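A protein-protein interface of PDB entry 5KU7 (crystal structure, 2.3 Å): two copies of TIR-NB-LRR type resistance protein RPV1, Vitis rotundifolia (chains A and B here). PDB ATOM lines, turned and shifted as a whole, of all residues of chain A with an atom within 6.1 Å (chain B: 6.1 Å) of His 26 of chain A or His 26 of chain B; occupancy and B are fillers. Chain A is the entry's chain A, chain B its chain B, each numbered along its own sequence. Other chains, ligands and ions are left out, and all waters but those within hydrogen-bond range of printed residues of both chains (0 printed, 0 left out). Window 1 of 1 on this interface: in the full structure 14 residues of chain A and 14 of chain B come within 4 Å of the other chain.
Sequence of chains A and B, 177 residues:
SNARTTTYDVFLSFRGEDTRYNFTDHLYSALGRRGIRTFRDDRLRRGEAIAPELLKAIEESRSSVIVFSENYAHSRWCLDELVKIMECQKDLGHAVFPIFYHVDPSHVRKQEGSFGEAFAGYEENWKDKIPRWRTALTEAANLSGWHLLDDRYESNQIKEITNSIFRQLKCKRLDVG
NE of Arg 33 of chain A lies close to NE of Arg 33 of chain B, at 3.3 Å. O of Tyr 21 of chain A lies within hydrogen-bond range of N of Glu 154 of chain B. The side-chain carboxylate (OD2) of Asp 25 of chain B sits at hydrogen-bond distance from the side-chain hydroxyl (OG) of Ser 155 of chain A (2.7 Å). The backbone NH (N) of Glu 154 of chain A lies within hydrogen-bond range of the side-chain carboxylate (OD2) of Asp 25 of chain B, at 3.4 Å. OD2 of Asp 25 of chain A is in hydrogen-bond range of OG of Ser 155 of chain B (2.8 Å). OE2 of Glu 154 of chain B lies within hydrogen-bond range of NE2 of His 26 of chain A. The backbone NH (N) of Glu 154 of chain B lies within hydrogen-bond range of the side-chain carboxylate (OD2) of Asp 25 of chain A, 3.2 Å away. The backbone carbonyl oxygen (O) of Tyr 21 of chain B lies within hydrogen-bond range of the backbone NH (N) of Glu 154 of chain A, at 2.9 Å. OE2 of Glu 154 of chain A lies within hydrogen-bond range of NE2 of His 26 of chain B (2.7 Å).
The side-chain hydroxyl (OG) of Ser 29 of chain A is in hydrogen-bond range of the guanidinium group (NH1) of Arg 33 of chain A, 3.0 Å away. NH1 of Arg 33 of chain B lies within hydrogen-bond range of OG of Ser 29 of chain B, 3.2 Å away.
Among the printed residues, merely in contact across the chains: His 26 of chain A with His 26 of chain B (3.3 Å), His 26 of chain A with Ser 155 of chain B (3.7 Å), His 26 of chain A with Ile 158 of chain B (3.9 Å), Ser 29 of chain A with Ser 155 of chain B (3.96 Å), Ser 155 of chain A with His 26 of chain B (3.7 Å), Ser 155 of chain A with Ser 29 of chain B (3.8 Å) and Ile 158 of chain A with His 26 of chain B (3.9 Å).
Of the printed residues of chain B, Asp 25 of chain A touches Glu 154 and Ser 155. Of chain B, only His 26, Glu 154, Ser 155 and Ile 158 come within 4 Å of His 26 of chain A. His 26 of chain B touches just these residues of chain A: His 26, Glu 154, Ser 155 and Ile 158. Printed residues of chain A within 4 Å of Ser 29 of chain B: Ser 155. The nearest residue of chain A that does not touch His 26 of chain B is Phe 23 of chain A (5.5 Å). The nearest printed residue of chain A that does not touch Ser 29 of chain B is Arg 33 of chain A (5.9 Å).
Hydrophobic or aromatic side chains of chain A within 4 Å of the printed part of chain B: His 26 and Ile 158. Among the printed residues, no Asp or Glu carboxylate lies within 4 Å of a Lys or Arg side-chain nitrogen of the other chain.
Asp 25 of chain A touches Glu 154 of chain B, and with the chains exchanged Glu 154 of chain A touches Asp 25 of chain B. Asp 25 of chain A touches Ser 155 of chain B, and with the chains exchanged Ser 155 of chain A touches Asp 25 of chain B. His 26 of chain A touches Glu 154 of chain B, and with the chains exchanged Glu 154 of chain A touches His 26 of chain B. Ser 29 of chain A touches Ser 155 of chain B, and with the chains exchanged Ser 155 of chain A touches Ser 29 of chain B. Of the 16 pairs that touch across the chains among the printed residues, 16 have their exchanged pair printed and touching as well.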
ATOM      1  N   ARG A  20     -15.153   3.849  27.905  1.00  0.00           N
ATOM      2  CA  ARG A  20     -15.327   3.600  26.470  1.00  0.00           C
ATOM      3  C   ARG A  20     -15.120   4.850  25.626  1.00  0.00           C
ATOM      4  O   ARG A  20     -14.383   4.845  24.638  1.00  0.00           O
ATOM      5  CB  ARG A  20     -16.728   3.068  26.143  1.00  0.00           C
ATOM      6  CG  ARG A  20     -16.975   2.970  24.612  1.00  0.00           C
ATOM      7  CD  ARG A  20     -18.340   2.318  24.281  1.00  0.00           C
ATOM      8  NE  ARG A  20     -18.378   0.904  24.640  1.00  0.00           N
ATOM      9  CZ  ARG A  20     -17.898  -0.078  23.888  1.00  0.00           C
ATOM     10  NH1 ARG A  20     -17.334   0.198  22.719  1.00  0.00           N
ATOM     11  NH2 ARG A  20     -17.975  -1.341  24.308  1.00  0.00           N
ATOM     12  N   TYR A  21     -15.805   5.915  26.011  1.00  0.00           N
ATOM     13  CA  TYR A  21     -15.879   7.086  25.179  1.00  0.00           C
ATOM     14  C   TYR A  21     -14.774   8.077  25.430  1.00  0.00           C
ATOM     15  O   TYR A  21     -14.608   9.008  24.656  1.00  0.00           O
ATOM     16  CB  TYR A  21     -17.233   7.768  25.364  1.00  0.00           C
ATOM     17  CG  TYR A  21     -18.335   6.894  24.867  1.00  0.00           C
ATOM     18  CD1 TYR A  21     -18.442   6.597  23.521  1.00  0.00           C
ATOM     19  CD2 TYR A  21     -19.238   6.311  25.747  1.00  0.00           C
ATOM     20  CE1 TYR A  21     -19.443   5.780  23.054  1.00  0.00           C
ATOM     21  CE2 TYR A  21     -20.245   5.499  25.291  1.00  0.00           C
ATOM     22  CZ  TYR A  21     -20.340   5.233  23.945  1.00  0.00           C
ATOM     23  OH  TYR A  21     -21.340   4.411  23.490  1.00  0.00           O
ATOM     24  N   ASN A  22     -14.020   7.902  26.508  1.00  0.00           N
ATOM     25  CA  ASN A  22     -12.976   8.881  26.779  1.00  0.00           C
ATOM     26  C   ASN A  22     -11.592   8.235  26.767  1.00  0.00           C
ATOM     27  O   ASN A  22     -10.974   8.140  25.700  1.00  0.00           O
ATOM     28  CB  ASN A  22     -13.266   9.639  28.095  1.00  0.00           C
ATOM     29  CG  ASN A  22     -13.945   8.766  29.147  1.00  0.00           C
ATOM     30  OD1 ASN A  22     -13.363   7.807  29.659  1.00  0.00           O
ATOM     31  ND2 ASN A  22     -15.170   9.127  29.502  1.00  0.00           N
ATOM     32  N   PHE A  23     -11.097   7.802  27.926  1.00  0.00           N
ATOM     33  CA  PHE A  23      -9.702   7.374  28.011  1.00  0.00           C
ATOM     34  C   PHE A  23      -9.316   6.277  27.020  1.00  0.00           C
ATOM     35  O   PHE A  23      -8.361   6.426  26.246  1.00  0.00           O
ATOM     36  CB  PHE A  23      -9.347   6.889  29.415  1.00  0.00           C
ATOM     37  CG  PHE A  23      -7.941   6.367  29.510  1.00  0.00           C
ATOM     38  CD1 PHE A  23      -6.864   7.256  29.587  1.00  0.00           C
ATOM     39  CD2 PHE A  23      -7.686   5.002  29.462  1.00  0.00           C
ATOM     40  CE1 PHE A  23      -5.566   6.786  29.658  1.00  0.00           C
ATOM     41  CE2 PHE A  23      -6.372   4.508  29.523  1.00  0.00           C
ATOM     42  CZ  PHE A  23      -5.309   5.395  29.620  1.00  0.00           C
ATOM     43  N   THR A  24     -10.059   5.183  27.036  1.00  0.00           N
ATOM     44  CA  THR A  24      -9.709   4.047  26.198  1.00  0.00           C
ATOM     45  C   THR A  24      -9.767   4.457  24.732  1.00  0.00           C
ATOM     46  O   THR A  24      -8.985   3.980  23.920  1.00  0.00           O
ATOM     47  CB  THR A  24     -10.645   2.855  26.448  1.00  0.00           C
ATOM     48  OG1 THR A  24     -10.583   2.483  27.834  1.00  0.00           O
ATOM     49  CG2 THR A  24     -10.229   1.692  25.601  1.00  0.00           C
ATOM     50  N   ASP A  25     -10.683   5.364  24.404  1.00  0.00           N
ATOM     51  CA  ASP A  25     -10.784   5.880  23.033  1.00  0.00           C
ATOM     52  C   ASP A  25      -9.531   6.659  22.633  1.00  0.00           C
ATOM     53  O   ASP A  25      -8.967   6.403  21.560  1.00  0.00           O
ATOM     54  CB  ASP A  25     -12.025   6.768  22.885  1.00  0.00           C
ATOM     55  CG  ASP A  25     -12.314   7.116  21.452  1.00  0.00           C
ATOM     56  OD1 ASP A  25     -12.135   6.240  20.598  1.00  0.00           O
ATOM     57  OD2 ASP A  25     -12.702   8.259  21.154  1.00  0.00           O
ATOM     58  N   HIS A  26      -9.086   7.576  23.508  1.00  0.00           N
ATOM     59  CA  HIS A  26      -7.848   8.355  23.279  1.00  0.00           C
ATOM     60  C   HIS A  26      -6.635   7.416  23.186  1.00  0.00           C
ATOM     61  O   HIS A  26      -5.730   7.628  22.367  1.00  0.00           O
ATOM     62  CB  HIS A  26      -7.626   9.403  24.391  1.00  0.00           C
ATOM     63  CG  HIS A  26      -8.675  10.480  24.430  1.00  0.00           C
ATOM     64  ND1 HIS A  26      -8.943  11.304  23.354  1.00  0.00           N
ATOM     65  CD2 HIS A  26      -9.528  10.856  25.411  1.00  0.00           C
ATOM     66  CE1 HIS A  26      -9.915  12.140  23.671  1.00  0.00           C
ATOM     67  NE2 HIS A  26     -10.291  11.884  24.910  1.00  0.00           N
ATOM     68  N   LEU A  27      -6.622   6.372  24.013  1.00  0.00           N
ATOM     69  CA  LEU A  27      -5.563   5.353  23.950  1.00  0.00           C
ATOM     70  C   LEU A  27      -5.578   4.623  22.608  1.00  0.00           C
ATOM     71  O   LEU A  27      -4.542   4.420  21.944  1.00  0.00           O
ATOM     72  CB  LEU A  27      -5.721   4.335  25.094  1.00  0.00           C
ATOM     73  CG  LEU A  27      -4.709   3.187  25.151  1.00  0.00           C
ATOM     74  CD1 LEU A  27      -3.309   3.721  25.384  1.00  0.00           C
ATOM     75  CD2 LEU A  27      -5.073   2.208  26.255  1.00  0.00           C
ATOM     76  N   TYR A  28      -6.780   4.205  22.238  1.00  0.00           N
ATOM     77  CA  TYR A  28      -7.027   3.515  20.990  1.00  0.00           C
ATOM     78  C   TYR A  28      -6.515   4.325  19.813  1.00  0.00           C
ATOM     79  O   TYR A  28      -5.837   3.816  18.923  1.00  0.00           O
ATOM     80  CB  TYR A  28      -8.532   3.241  20.847  1.00  0.00           C
ATOM     81  CG  TYR A  28      -8.923   2.685  19.503  1.00  0.00           C
ATOM     82  CD1 TYR A  28      -8.491   1.418  19.106  1.00  0.00           C
ATOM     83  CD2 TYR A  28      -9.703   3.427  18.618  1.00  0.00           C
ATOM     84  CE1 TYR A  28      -8.845   0.887  17.873  1.00  0.00           C
ATOM     85  CE2 TYR A  28     -10.069   2.896  17.370  1.00  0.00           C
ATOM     86  CZ  TYR A  28      -9.628   1.624  17.006  1.00  0.00           C
ATOM     87  OH  TYR A  28      -9.963   1.070  15.787  1.00  0.00           O
ATOM     88  N   SER A  29      -6.872   5.596  19.803  1.00  0.00           N
ATOM     89  CA  SER A  29      -6.473   6.455  18.706  1.00  0.00           C
ATOM     90  C   SER A  29      -4.955   6.642  18.713  1.00  0.00           C
ATOM     91  O   SER A  29      -4.325   6.609  17.657  1.00  0.00           O
ATOM     92  CB  SER A  29      -7.193   7.798  18.811  1.00  0.00           C
ATOM     93  OG  SER A  29      -6.775   8.682  17.793  1.00  0.00           O
ATOM     94  N   ALA A  30      -4.366   6.807  19.902  1.00  0.00           N
ATOM     95  CA  ALA A  30      -2.907   6.969  20.013  1.00  0.00           C
ATOM     96  C   ALA A  30      -2.170   5.739  19.486  1.00  0.00           C
ATOM     97  O   ALA A  30      -1.143   5.868  18.819  1.00  0.00           O
ATOM     98  CB  ALA A  30      -2.506   7.247  21.455  1.00  0.00           C
ATOM     99  N   LEU A  31      -2.691   4.545  19.785  1.00  0.00           N
ATOM    100  CA  LEU A  31      -2.051   3.307  19.315  1.00  0.00           C
ATOM    101  C   LEU A  31      -2.036   3.269  17.795  1.00  0.00           C
ATOM    102  O   LEU A  31      -1.032   2.911  17.179  1.00  0.00           O
ATOM    103  CB  LEU A  31      -2.766   2.072  19.867  1.00  0.00           C
ATOM    104  CG  LEU A  31      -2.640   1.885  21.385  1.00  0.00           C
ATOM    105  CD1 LEU A  31      -3.692   0.898  21.839  1.00  0.00           C
ATOM    106  CD2 LEU A  31      -1.230   1.404  21.779  1.00  0.00           C
ATOM    107  N   ARG A  33      -2.092   5.710  15.712  1.00  0.00           N
ATOM    108  CA  ARG A  33      -1.148   6.678  15.174  1.00  0.00           C
ATOM    109  C   ARG A  33       0.267   6.120  15.082  1.00  0.00           C
ATOM    110  O   ARG A  33       1.057   6.569  14.257  1.00  0.00           O
ATOM    111  CB  ARG A  33      -1.161   7.965  16.011  1.00  0.00           C
ATOM    112  CG  ARG A  33      -2.385   8.830  15.740  1.00  0.00           C
ATOM    113  CD  ARG A  33      -2.186  10.273  16.220  1.00  0.00           C
ATOM    114  NE  ARG A  33      -2.004  10.342  17.667  1.00  0.00           N
ATOM    115  CZ  ARG A  33      -3.004  10.329  18.537  1.00  0.00           C
ATOM    116  NH1 ARG A  33      -4.267  10.256  18.102  1.00  0.00           N
ATOM    117  NH2 ARG A  33      -2.748  10.389  19.837  1.00  0.00           N
ATOM    118  N   ARG A  40     -10.527  -2.832  19.070  1.00  0.00           N
ATOM    119  CA  ARG A  40     -11.320  -2.177  20.099  1.00  0.00           C
ATOM    120  C   ARG A  40     -12.794  -2.391  19.832  1.00  0.00           C
ATOM    121  O   ARG A  40     -13.330  -1.810  18.895  1.00  0.00           O
ATOM    122  CB  ARG A  40     -10.983  -0.679  20.159  1.00  0.00           C
ATOM    123  CG  ARG A  40     -11.695   0.040  21.272  1.00  0.00           C
ATOM    124  CD  ARG A  40     -13.060   0.513  20.785  1.00  0.00           C
ATOM    125  NE  ARG A  40     -13.112   1.946  21.023  1.00  0.00           N
ATOM    126  CZ  ARG A  40     -12.985   2.876  20.094  1.00  0.00           C
ATOM    127  NH1 ARG A  40     -12.880   2.551  18.818  1.00  0.00           N
ATOM    128  NH2 ARG A  40     -13.004   4.143  20.455  1.00  0.00           N
ATOM    129  N   GLU A 154      -3.218  13.773  30.888  1.00  0.00           N
ATOM    130  CA  GLU A 154      -3.581  12.439  30.406  1.00  0.00           C
ATOM    131  C   GLU A 154      -2.980  12.117  29.042  1.00  0.00           C
ATOM    132  O   GLU A 154      -2.630  10.975  28.788  1.00  0.00           O
ATOM    133  CB  GLU A 154      -5.097  12.275  30.378  1.00  0.00           C
ATOM    134  CG  GLU A 154      -5.560  10.798  30.266  1.00  0.00           C
ATOM    135  CD  GLU A 154      -7.049  10.661  30.504  1.00  0.00           C
ATOM    136  OE1 GLU A 154      -7.434  10.346  31.656  1.00  0.00           O
ATOM    137  OE2 GLU A 154      -7.838  10.894  29.544  1.00  0.00           O
ATOM    138  N   SER A 155      -2.836  13.104  28.161  1.00  0.00           N
ATOM    139  CA  SER A 155      -2.245  12.806  26.855  1.00  0.00           C
ATOM    140  C   SER A 155      -0.779  12.383  26.996  1.00  0.00           C
ATOM    141  O   SER A 155      -0.262  11.604  26.199  1.00  0.00           O
ATOM    142  CB  SER A 155      -2.363  13.999  25.905  1.00  0.00           C
ATOM    143  OG  SER A 155      -1.444  15.005  26.258  1.00  0.00           O
ATOM    144  N   ILE A 158      -0.713   8.856  28.145  1.00  0.00           N
ATOM    145  CA  ILE A 158      -0.984   8.020  26.987  1.00  0.00           C
ATOM    146  C   ILE A 158       0.208   7.925  26.032  1.00  0.00           C
ATOM    147  O   ILE A 158       0.489   6.856  25.495  1.00  0.00           O
ATOM    148  CB  ILE A 158      -2.200   8.540  26.204  1.00  0.00           C
ATOM    149  CG1 ILE A 158      -3.485   8.256  26.981  1.00  0.00           C
ATOM    150  CG2 ILE A 158      -2.237   7.912  24.811  1.00  0.00           C
ATOM    151  CD1 ILE A 158      -4.736   8.413  26.158  1.00  0.00           C
ATOM    152  N   ARG B  20      -8.619  20.580  32.688  1.00  0.00           N
ATOM    153  CA  ARG B  20      -7.185  20.747  32.434  1.00  0.00           C
ATOM    154  C   ARG B  20      -6.468  19.452  32.081  1.00  0.00           C
ATOM    155  O   ARG B  20      -5.742  19.412  31.094  1.00  0.00           O
ATOM    156  CB  ARG B  20      -6.425  21.388  33.613  1.00  0.00           C
ATOM    157  CG  ARG B  20      -4.882  21.160  33.439  1.00  0.00           C
ATOM    158  CD  ARG B  20      -3.915  21.925  34.370  1.00  0.00           C
ATOM    159  NE  ARG B  20      -3.759  23.341  33.989  1.00  0.00           N
ATOM    160  CZ  ARG B  20      -4.458  24.283  34.571  1.00  0.00           C
ATOM    161  NH1 ARG B  20      -5.290  23.907  35.526  1.00  0.00           N
ATOM    162  NH2 ARG B  20      -4.339  25.559  34.232  1.00  0.00           N
ATOM    163  N   TYR B  21      -6.653  18.416  32.884  1.00  0.00           N
ATOM    164  CA  TYR B  21      -5.825  17.228  32.738  1.00  0.00           C
ATOM    165  C   TYR B  21      -6.378  16.191  31.757  1.00  0.00           C
ATOM    166  O   TYR B  21      -5.653  15.273  31.378  1.00  0.00           O
ATOM    167  CB  TYR B  21      -5.616  16.571  34.110  1.00  0.00           C
ATOM    168  CG  TYR B  21      -4.854  17.463  35.040  1.00  0.00           C
ATOM    169  CD1 TYR B  21      -3.525  17.783  34.779  1.00  0.00           C
ATOM    170  CD2 TYR B  21      -5.469  18.038  36.146  1.00  0.00           C
ATOM    171  CE1 TYR B  21      -2.824  18.610  35.596  1.00  0.00           C
ATOM    172  CE2 TYR B  21      -4.774  18.883  36.975  1.00  0.00           C
ATOM    173  CZ  TYR B  21      -3.446  19.168  36.699  1.00  0.00           C
ATOM    174  OH  TYR B  21      -2.728  20.016  37.520  1.00  0.00           O
ATOM    175  N   ASN B  22      -7.636  16.327  31.337  1.00  0.00           N
ATOM    176  CA  ASN B  22      -8.214  15.342  30.412  1.00  0.00           C
ATOM    177  C   ASN B  22      -8.621  15.994  29.090  1.00  0.00           C
ATOM    178  O   ASN B  22      -7.776  16.160  28.217  1.00  0.00           O
ATOM    179  CB  ASN B  22      -9.404  14.619  31.058  1.00  0.00           C
ATOM    180  CG  ASN B  22     -10.239  15.546  31.917  1.00  0.00           C
ATOM    181  OD1 ASN B  22     -10.897  16.451  31.400  1.00  0.00           O
ATOM    182  ND2 ASN B  22     -10.185  15.357  33.233  1.00  0.00           N
ATOM    183  N   PHE B  23      -9.882  16.403  28.932  1.00  0.00           N
ATOM    184  CA  PHE B  23     -10.343  16.835  27.602  1.00  0.00           C
ATOM    185  C   PHE B  23      -9.491  17.916  26.953  1.00  0.00           C
ATOM    186  O   PHE B  23      -9.077  17.799  25.799  1.00  0.00           O
ATOM    187  CB  PHE B  23     -11.775  17.366  27.630  1.00  0.00           C
ATOM    188  CG  PHE B  23     -12.219  17.924  26.297  1.00  0.00           C
ATOM    189  CD1 PHE B  23     -12.619  17.074  25.275  1.00  0.00           C
ATOM    190  CD2 PHE B  23     -12.189  19.287  26.052  1.00  0.00           C
ATOM    191  CE1 PHE B  23     -13.016  17.575  24.042  1.00  0.00           C
ATOM    192  CE2 PHE B  23     -12.583  19.803  24.812  1.00  0.00           C
ATOM    193  CZ  PHE B  23     -12.999  18.945  23.811  1.00  0.00           C
ATOM    194  N   THR B  24      -9.262  18.992  27.675  1.00  0.00           N
ATOM    195  CA  THR B  24      -8.511  20.088  27.100  1.00  0.00           C
ATOM    196  C   THR B  24      -7.069  19.667  26.799  1.00  0.00           C
ATOM    197  O   THR B  24      -6.481  20.097  25.802  1.00  0.00           O
ATOM    198  CB  THR B  24      -8.566  21.317  28.038  1.00  0.00           C
ATOM    199  OG1 THR B  24      -9.943  21.662  28.236  1.00  0.00           O
ATOM    200  CG2 THR B  24      -7.815  22.506  27.443  1.00  0.00           C
ATOM    201  N   ASP B  25      -6.497  18.796  27.625  1.00  0.00           N
ATOM    202  CA  ASP B  25      -5.153  18.296  27.315  1.00  0.00           C
ATOM    203  C   ASP B  25      -5.138  17.464  26.004  1.00  0.00           C
ATOM    204  O   ASP B  25      -4.250  17.602  25.142  1.00  0.00           O
ATOM    205  CB  ASP B  25      -4.595  17.462  28.477  1.00  0.00           C
ATOM    206  CG  ASP B  25      -3.104  17.203  28.329  1.00  0.00           C
ATOM    207  OD1 ASP B  25      -2.380  18.192  28.046  1.00  0.00           O
ATOM    208  OD2 ASP B  25      -2.668  16.031  28.455  1.00  0.00           O
ATOM    209  N   HIS B  26      -6.119  16.593  25.847  1.00  0.00           N
ATOM    210  CA  HIS B  26      -6.207  15.813  24.613  1.00  0.00           C
ATOM    211  C   HIS B  26      -6.412  16.719  23.401  1.00  0.00           C
ATOM    212  O   HIS B  26      -5.867  16.468  22.323  1.00  0.00           O
ATOM    213  CB  HIS B  26      -7.339  14.785  24.701  1.00  0.00           C
ATOM    214  CG  HIS B  26      -7.108  13.723  25.716  1.00  0.00           C
ATOM    215  ND1 HIS B  26      -6.009  12.892  25.680  1.00  0.00           N
ATOM    216  CD2 HIS B  26      -7.837  13.337  26.791  1.00  0.00           C
ATOM    217  CE1 HIS B  26      -6.073  12.036  26.687  1.00  0.00           C
ATOM    218  NE2 HIS B  26      -7.182  12.274  27.366  1.00  0.00           N
ATOM    219  N   LEU B  27      -7.214  17.766  23.589  1.00  0.00           N
ATOM    220  CA  LEU B  27      -7.440  18.783  22.556  1.00  0.00           C
ATOM    221  C   LEU B  27      -6.160  19.531  22.223  1.00  0.00           C
ATOM    222  O   LEU B  27      -5.796  19.686  21.047  1.00  0.00           O
ATOM    223  CB  LEU B  27      -8.509  19.779  23.008  1.00  0.00           C
ATOM    224  CG  LEU B  27      -8.769  20.940  22.050  1.00  0.00           C
ATOM    225  CD1 LEU B  27      -9.363  20.416  20.732  1.00  0.00           C
ATOM    226  CD2 LEU B  27      -9.667  22.017  22.697  1.00  0.00           C
ATOM    227  N   TYR B  28      -5.480  19.992  23.269  1.00  0.00           N
ATOM    228  CA  TYR B  28      -4.204  20.687  23.117  1.00  0.00           C
ATOM    229  C   TYR B  28      -3.231  19.868  22.290  1.00  0.00           C
ATOM    230  O   TYR B  28      -2.630  20.346  21.336  1.00  0.00           O
ATOM    231  CB  TYR B  28      -3.592  20.959  24.490  1.00  0.00           C
ATOM    232  CG  TYR B  28      -2.191  21.542  24.453  1.00  0.00           C
ATOM    233  CD1 TYR B  28      -1.964  22.798  23.917  1.00  0.00           C
ATOM    234  CD2 TYR B  28      -1.107  20.851  24.980  1.00  0.00           C
ATOM    235  CE1 TYR B  28      -0.699  23.356  23.897  1.00  0.00           C
ATOM    236  CE2 TYR B  28       0.174  21.404  24.960  1.00  0.00           C
ATOM    237  CZ  TYR B  28       0.360  22.671  24.419  1.00  0.00           C
ATOM    238  OH  TYR B  28       1.605  23.256  24.379  1.00  0.00           O
ATOM    239  N   SER B  29      -3.099  18.605  22.664  1.00  0.00           N
ATOM    240  CA  SER B  29      -2.150  17.733  22.008  1.00  0.00           C
ATOM    241  C   SER B  29      -2.594  17.461  20.552  1.00  0.00           C
ATOM    242  O   SER B  29      -1.771  17.434  19.630  1.00  0.00           O
ATOM    243  CB  SER B  29      -1.985  16.458  22.838  1.00  0.00           C
ATOM    244  OG  SER B  29      -1.089  15.570  22.224  1.00  0.00           O
ATOM    245  N   ALA B  30      -3.895  17.292  20.335  1.00  0.00           N
ATOM    246  CA  ALA B  30      -4.390  17.063  18.972  1.00  0.00           C
ATOM    247  C   ALA B  30      -4.066  18.275  18.090  1.00  0.00           C
ATOM    248  O   ALA B  30      -3.636  18.131  16.952  1.00  0.00           O
ATOM    249  CB  ALA B  30      -5.877  16.775  18.971  1.00  0.00           C
ATOM    250  N   LEU B  31      -4.221  19.473  18.630  1.00  0.00           N
ATOM    251  CA  LEU B  31      -3.920  20.657  17.831  1.00  0.00           C
ATOM    252  C   LEU B  31      -2.464  20.673  17.384  1.00  0.00           C
ATOM    253  O   LEU B  31      -2.175  20.865  16.206  1.00  0.00           O
ATOM    254  CB  LEU B  31      -4.238  21.934  18.610  1.00  0.00           C
ATOM    255  CG  LEU B  31      -5.712  22.216  18.884  1.00  0.00           C
ATOM    256  CD1 LEU B  31      -5.848  23.309  19.952  1.00  0.00           C
ATOM    257  CD2 LEU B  31      -6.397  22.639  17.591  1.00  0.00           C
ATOM    258  N   ARG B  33      -0.325  18.194  17.045  1.00  0.00           N
ATOM    259  CA  ARG B  33      -0.025  17.157  16.072  1.00  0.00           C
ATOM    260  C   ARG B  33      -0.337  17.667  14.663  1.00  0.00           C
ATOM    261  O   ARG B  33       0.294  17.249  13.689  1.00  0.00           O
ATOM    262  CB  ARG B  33      -0.831  15.870  16.349  1.00  0.00           C
ATOM    263  CG  ARG B  33      -0.325  15.062  17.516  1.00  0.00           C
ATOM    264  CD  ARG B  33      -0.857  13.617  17.470  1.00  0.00           C
ATOM    265  NE  ARG B  33      -2.314  13.579  17.544  1.00  0.00           N
ATOM    266  CZ  ARG B  33      -3.020  13.690  18.666  1.00  0.00           C
ATOM    267  NH1 ARG B  33      -2.407  13.875  19.834  1.00  0.00           N
ATOM    268  NH2 ARG B  33      -4.348  13.642  18.613  1.00  0.00           N
ATOM    269  N   GLU B 154     -14.815  10.412  22.138  1.00  0.00           N
ATOM    270  CA  GLU B 154     -14.250  11.733  22.351  1.00  0.00           C
ATOM    271  C   GLU B 154     -13.105  12.061  21.371  1.00  0.00           C
ATOM    272  O   GLU B 154     -13.012  13.193  20.897  1.00  0.00           O
ATOM    273  CB  GLU B 154     -13.785  11.858  23.792  1.00  0.00           C
ATOM    274  CG  GLU B 154     -13.581  13.319  24.213  1.00  0.00           C
ATOM    275  CD  GLU B 154     -13.368  13.470  25.693  1.00  0.00           C
ATOM    276  OE1 GLU B 154     -14.344  13.777  26.422  1.00  0.00           O
ATOM    277  OE2 GLU B 154     -12.216  13.286  26.123  1.00  0.00           O
ATOM    278  N   SER B 155     -12.287  11.079  21.004  1.00  0.00           N
ATOM    279  CA  SER B 155     -11.219  11.348  20.042  1.00  0.00           C
ATOM    280  C   SER B 155     -11.794  11.711  18.679  1.00  0.00           C
ATOM    281  O   SER B 155     -11.163  12.452  17.934  1.00  0.00           O
ATOM    282  CB  SER B 155     -10.276  10.154  19.900  1.00  0.00           C
ATOM    283  OG  SER B 155     -10.912   9.127  19.159  1.00  0.00           O
ATOM    284  N   ILE B 158     -12.809  15.278  18.924  1.00  0.00           N
ATOM    285  CA  ILE B 158     -11.651  16.171  18.880  1.00  0.00           C
ATOM    286  C   ILE B 158     -11.105  16.299  17.458  1.00  0.00           C
ATOM    287  O   ILE B 158     -10.743  17.395  17.013  1.00  0.00           O
ATOM    288  CB  ILE B 158     -10.517  15.707  19.849  1.00  0.00           C
ATOM    289  CG1 ILE B 158     -10.964  15.899  21.301  1.00  0.00           C
ATOM    290  CG2 ILE B 158      -9.236  16.444  19.551  1.00  0.00           C
ATOM    291  CD1 ILE B 158      -9.846  15.821  22.365  1.00  0.00           C
